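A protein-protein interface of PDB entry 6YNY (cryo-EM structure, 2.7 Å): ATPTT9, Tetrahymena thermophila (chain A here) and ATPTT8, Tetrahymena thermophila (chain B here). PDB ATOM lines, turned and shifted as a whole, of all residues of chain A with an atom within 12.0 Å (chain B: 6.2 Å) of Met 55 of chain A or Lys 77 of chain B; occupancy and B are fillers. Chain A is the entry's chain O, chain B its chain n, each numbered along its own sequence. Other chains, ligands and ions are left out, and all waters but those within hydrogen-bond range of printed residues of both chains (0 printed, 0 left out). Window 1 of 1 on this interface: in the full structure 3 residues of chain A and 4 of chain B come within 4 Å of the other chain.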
ATOM      1  N   MET A  55      17.121  31.803  19.944  1.00  0.00           N
ATOM      2  CA  MET A  55      18.268  32.140  20.776  1.00  0.00           C
ATOM      3  C   MET A  55      18.298  33.639  21.058  1.00  0.00           C
ATOM      4  O   MET A  55      18.296  34.447  20.132  1.00  0.00           O
ATOM      5  CB  MET A  55      19.554  31.707  20.091  1.00  0.00           C
ATOM      6  CG  MET A  55      20.759  31.673  21.007  1.00  0.00           C
ATOM      7  SD  MET A  55      20.718  30.274  22.128  1.00  0.00           S
ATOM      8  CE  MET A  55      22.293  30.470  22.942  1.00  0.00           C
ATOM      9  N   GLN A  56      18.329  34.007  22.339  1.00  0.00           N
ATOM     10  CA  GLN A  56      18.312  35.414  22.714  1.00  0.00           C
ATOM     11  C   GLN A  56      19.421  36.177  22.007  1.00  0.00           C
ATOM     12  O   GLN A  56      20.578  35.749  21.986  1.00  0.00           O
ATOM     13  CB  GLN A  56      18.460  35.569  24.225  1.00  0.00           C
ATOM     14  CG  GLN A  56      17.240  35.199  25.025  1.00  0.00           C
ATOM     15  CD  GLN A  56      17.240  33.757  25.466  1.00  0.00           C
ATOM     16  OE1 GLN A  56      17.805  32.888  24.804  1.00  0.00           O
ATOM     17  NE2 GLN A  56      16.621  33.496  26.604  1.00  0.00           N
ATOM     18  N   ASN A  57      19.055  37.321  21.432  1.00  0.00           N
ATOM     19  CA  ASN A  57      19.999  38.094  20.636  1.00  0.00           C
ATOM     20  C   ASN A  57      21.053  38.757  21.511  1.00  0.00           C
ATOM     21  O   ASN A  57      22.218  38.870  21.111  1.00  0.00           O
ATOM     22  CB  ASN A  57      19.244  39.130  19.810  1.00  0.00           C
ATOM     23  CG  ASN A  57      18.335  39.998  20.653  1.00  0.00           C
ATOM     24  OD1 ASN A  57      18.024  39.665  21.795  1.00  0.00           O
ATOM     25  ND2 ASN A  57      17.896  41.111  20.090  1.00  0.00           N
ATOM     26  N   THR A  58      20.667  39.212  22.697  1.00  0.00           N
ATOM     27  CA  THR A  58      21.587  39.872  23.619  1.00  0.00           C
ATOM     28  C   THR A  58      22.212  38.876  24.592  1.00  0.00           C
ATOM     29  O   THR A  58      22.211  39.075  25.804  1.00  0.00           O
ATOM     30  CB  THR A  58      20.860  40.979  24.371  1.00  0.00           C
ATOM     31  OG1 THR A  58      19.876  40.406  25.239  1.00  0.00           O
ATOM     32  CG2 THR A  58      20.185  41.938  23.416  1.00  0.00           C
ATOM     33  N   THR A  59      22.766  37.795  24.056  1.00  0.00           N
ATOM     34  CA  THR A  59      23.385  36.741  24.847  1.00  0.00           C
ATOM     35  C   THR A  59      24.893  36.792  24.664  1.00  0.00           C
ATOM     36  O   THR A  59      25.383  36.901  23.536  1.00  0.00           O
ATOM     37  CB  THR A  59      22.850  35.368  24.446  1.00  0.00           C
ATOM     38  OG1 THR A  59      21.466  35.275  24.791  1.00  0.00           O
ATOM     39  CG2 THR A  59      23.612  34.268  25.145  1.00  0.00           C
ATOM     40  N   ASN A  60      25.621  36.709  25.773  1.00  0.00           N
ATOM     41  CA  ASN A  60      27.070  36.786  25.765  1.00  0.00           C
ATOM     42  C   ASN A  60      27.644  35.742  26.708  1.00  0.00           C
ATOM     43  O   ASN A  60      27.101  35.507  27.790  1.00  0.00           O
ATOM     44  CB  ASN A  60      27.556  38.177  26.184  1.00  0.00           C
ATOM     45  CG  ASN A  60      27.011  39.277  25.303  1.00  0.00           C
ATOM     46  OD1 ASN A  60      26.581  40.319  25.790  1.00  0.00           O
ATOM     47  ND2 ASN A  60      27.020  39.051  23.999  1.00  0.00           N
ATOM     48  N   ILE A  61      28.742  35.123  26.289  1.00  0.00           N
ATOM     49  CA  ILE A  61      29.470  34.157  27.102  1.00  0.00           C
ATOM     50  C   ILE A  61      30.751  34.831  27.567  1.00  0.00           C
ATOM     51  O   ILE A  61      31.606  35.186  26.748  1.00  0.00           O
ATOM     52  CB  ILE A  61      29.786  32.871  26.327  1.00  0.00           C
ATOM     53  CG1 ILE A  61      28.524  32.284  25.696  1.00  0.00           C
ATOM     54  CG2 ILE A  61      30.418  31.859  27.250  1.00  0.00           C
ATOM     55  CD1 ILE A  61      27.552  31.726  26.672  1.00  0.00           C
ATOM     56  N   VAL A  62      30.887  35.002  28.876  1.00  0.00           N
ATOM     57  CA  VAL A  62      32.035  35.669  29.472  1.00  0.00           C
ATOM     58  C   VAL A  62      32.878  34.633  30.195  1.00  0.00           C
ATOM     59  O   VAL A  62      32.346  33.719  30.832  1.00  0.00           O
ATOM     60  CB  VAL A  62      31.597  36.793  30.429  1.00  0.00           C
ATOM     61  CG1 VAL A  62      32.789  37.594  30.877  1.00  0.00           C
ATOM     62  CG2 VAL A  62      30.590  37.693  29.753  1.00  0.00           C
ATOM     63  N   TYR B  74      21.762  26.360  28.671  1.00  0.00           N
ATOM     64  CA  TYR B  74      22.175  25.887  27.360  1.00  0.00           C
ATOM     65  C   TYR B  74      23.026  26.933  26.656  1.00  0.00           C
ATOM     66  O   TYR B  74      22.780  28.137  26.769  1.00  0.00           O
ATOM     67  CB  TYR B  74      20.955  25.550  26.508  1.00  0.00           C
ATOM     68  CG  TYR B  74      20.031  24.532  27.117  1.00  0.00           C
ATOM     69  CD1 TYR B  74      20.526  23.437  27.802  1.00  0.00           C
ATOM     70  CD2 TYR B  74      18.659  24.668  27.012  1.00  0.00           C
ATOM     71  CE1 TYR B  74      19.682  22.511  28.360  1.00  0.00           C
ATOM     72  CE2 TYR B  74      17.811  23.747  27.564  1.00  0.00           C
ATOM     73  CZ  TYR B  74      18.324  22.669  28.237  1.00  0.00           C
ATOM     74  OH  TYR B  74      17.469  21.749  28.789  1.00  0.00           O
ATOM     75  N   ARG B  75      24.031  26.465  25.919  1.00  0.00           N
ATOM     76  CA  ARG B  75      24.920  27.362  25.195  1.00  0.00           C
ATOM     77  C   ARG B  75      24.493  27.563  23.748  1.00  0.00           C
ATOM     78  O   ARG B  75      24.602  28.675  23.222  1.00  0.00           O
ATOM     79  CB  ARG B  75      26.351  26.829  25.228  1.00  0.00           C
ATOM     80  CG  ARG B  75      27.376  27.856  24.800  1.00  0.00           C
ATOM     81  CD  ARG B  75      28.662  27.228  24.355  1.00  0.00           C
ATOM     82  NE  ARG B  75      29.577  28.231  23.819  1.00  0.00           N
ATOM     83  CZ  ARG B  75      30.625  28.730  24.465  1.00  0.00           C
ATOM     84  NH1 ARG B  75      30.931  28.330  25.690  1.00  0.00           N
ATOM     85  NH2 ARG B  75      31.378  29.639  23.871  1.00  0.00           N
ATOM     86  N   ASN B  76      24.016  26.509  23.088  1.00  0.00           N
ATOM     87  CA  ASN B  76      23.590  26.577  21.697  1.00  0.00           C
ATOM     88  C   ASN B  76      22.080  26.458  21.544  1.00  0.00           C
ATOM     89  O   ASN B  76      21.595  26.137  20.456  1.00  0.00           O
ATOM     90  CB  ASN B  76      24.293  25.499  20.877  1.00  0.00           C
ATOM     91  CG  ASN B  76      25.773  25.755  20.727  1.00  0.00           C
ATOM     92  OD1 ASN B  76      26.234  26.890  20.828  1.00  0.00           O
ATOM     93  ND2 ASN B  76      26.529  24.700  20.472  1.00  0.00           N
ATOM     94  N   LYS B  77      21.327  26.707  22.611  1.00  0.00           N
ATOM     95  CA  LYS B  77      19.877  26.639  22.573  1.00  0.00           C
ATOM     96  C   LYS B  77      19.301  27.745  23.439  1.00  0.00           C
ATOM     97  O   LYS B  77      19.912  28.170  24.421  1.00  0.00           O
ATOM     98  CB  LYS B  77      19.360  25.282  23.055  1.00  0.00           C
ATOM     99  CG  LYS B  77      19.583  24.155  22.081  1.00  0.00           C
ATOM    100  CD  LYS B  77      19.675  22.822  22.788  1.00  0.00           C
ATOM    101  CE  LYS B  77      18.457  22.549  23.626  1.00  0.00           C
ATOM    102  NZ  LYS B  77      18.606  21.292  24.390  1.00  0.00           N
ATOM    103  N   ALA B  78      18.116  28.209  23.058  1.00  0.00           N
ATOM    104  CA  ALA B  78      17.446  29.249  23.819  1.00  0.00           C
ATOM    105  C   ALA B  78      17.174  28.784  25.243  1.00  0.00           C
ATOM    106  O   ALA B  78      16.783  27.639  25.480  1.00  0.00           O
ATOM    107  CB  ALA B  78      16.141  29.639  23.138  1.00  0.00           C
ATOM    108  N   ASN B  79      17.385  29.686  26.192  1.00  0.00           N
ATOM    109  CA  ASN B  79      17.200  29.397  27.607  1.00  0.00           C
ATOM    110  C   ASN B  79      15.819  29.891  28.013  1.00  0.00           C
ATOM    111  O   ASN B  79      15.605  31.088  28.211  1.00  0.00           O
ATOM    112  CB  ASN B  79      18.301  30.038  28.438  1.00  0.00           C
ATOM    113  CG  ASN B  79      19.605  29.295  28.330  1.00  0.00           C
ATOM    114  OD1 ASN B  79      19.880  28.386  29.109  1.00  0.00           O
ATOM    115  ND2 ASN B  79      20.411  29.665  27.355  1.00  0.00           N
ATOM    116  N   GLN B 154      20.113  14.802  31.167  1.00  0.00           N
ATOM    117  CA  GLN B 154      20.700  15.618  30.114  1.00  0.00           C
ATOM    118  C   GLN B 154      22.136  15.998  30.446  1.00  0.00           C
ATOM    119  O   GLN B 154      22.952  16.199  29.543  1.00  0.00           O
ATOM    120  CB  GLN B 154      19.843  16.864  29.899  1.00  0.00           C
ATOM    121  CG  GLN B 154      20.178  17.655  28.663  1.00  0.00           C
ATOM    122  CD  GLN B 154      19.214  18.790  28.432  1.00  0.00           C
ATOM    123  OE1 GLN B 154      18.411  19.124  29.299  1.00  0.00           O
ATOM    124  NE2 GLN B 154      19.282  19.385  27.254  1.00  0.00           N
ATOM    125  N   HIS B 161      25.613  20.153  25.815  1.00  0.00           N
ATOM    126  CA  HIS B 161      24.539  21.117  25.632  1.00  0.00           C
ATOM    127  C   HIS B 161      24.668  22.326  26.544  1.00  0.00           C
ATOM    128  O   HIS B 161      24.101  23.378  26.235  1.00  0.00           O
ATOM    129  CB  HIS B 161      23.187  20.453  25.894  1.00  0.00           C
ATOM    130  CG  HIS B 161      22.738  19.531  24.808  1.00  0.00           C
ATOM    131  ND1 HIS B 161      21.535  18.863  24.859  1.00  0.00           N
ATOM    132  CD2 HIS B 161      23.320  19.171  23.641  1.00  0.00           C
ATOM    133  CE1 HIS B 161      21.396  18.129  23.772  1.00  0.00           C
ATOM    134  NE2 HIS B 161      22.467  18.296  23.016  1.00  0.00           N
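Arg 75 of chain B touches Met 55 of chain A. OE1 of Gln 56 of chain A touches CA of Ala 78 of chain B (3.8 Å). Ile 61 of chain A touches Arg 75 of chain B (CG2 to NH1, 3.9 Å).
Of the 8 printed residues of chain B, 4 touch a printed residue of chain A. Along chain B the printed residues that touch a printed residue of chain A span positions 75 to 79. Of the 8 printed residues of chain A, 3 touch a printed residue of chain B. Hydrophobic or aromatic side chains of chain A within 4 Å of the printed part of chain B: Met 55 and Ile 61. Among the printed residues, 6 pairs touch across the chains.
N of Lys 77 of chain B lies close to SD of Met 55 of chain A (3.7 Å). The backbone NH (N) of Ala 78 of chain B is in hydrogen-bond range of the side-chain sulfur (SD) of Met 55 of chain A, 3.4 Å away. O of Asn 79 of chain B lies within hydrogen-bond range of NE2 of Gln 56 of chain A.
The side-chain amide oxygen (OD1) of Asn 79 of chain B sits at hydrogen-bond distance from the backbone NH (N) of Tyr 74 of chain B (2.8 Å). The backbone NH of Arg 75 of chain B lies within hydrogen-bond range of the backbone carbonyl oxygen of His 161 of chain B, at 3.1 Å. ND2 of Asn 79 of chain B is in hydrogen-bond range of O of Lys 77 of chain B (3.3 Å). The backbone carbonyl oxygen (O) of Gln 56 of chain A is in hydrogen-bond range of the side-chain hydroxyl (OG1) of Thr 59 of chain A, at 3.0 Å.
Of chain B, only Arg 75 (2.9 Å), Lys 77 (3.2 Å) and Ala 78 (3.4 Å) come within 4 Å of Met 55 of chain A. Of the printed residues of chain A, Lys 77 of chain B touches Met 55. No residue of chain A comes within 4 Å of Tyr 74 of chain B. No residue of chain A comes within 4 Å of Asn 76 of chain B. Ala 78 of chain B touches just these residues of chain A: Met 55 and Gln 56. Of chain A, only Gln 56 comes within 4 Å of Asn 79 of chain B. Printed residues of chain A within 4 Å of Arg 75 of chain B: Met 55 (2.9 Å) and Ile 61 (3.9 Å). Of the printed residues of chain B, Ile 61 of chain A touches Arg 75. Of the printed residues of chain B, Gln 56 of chain A touches Ala 78 and Asn 79. Val 62 of chain A touches none of the printed residues of chain B. The nearest residue of chain A that does not touch Lys 77 of chain B is Gln 56 of chain A (5.2 Å).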
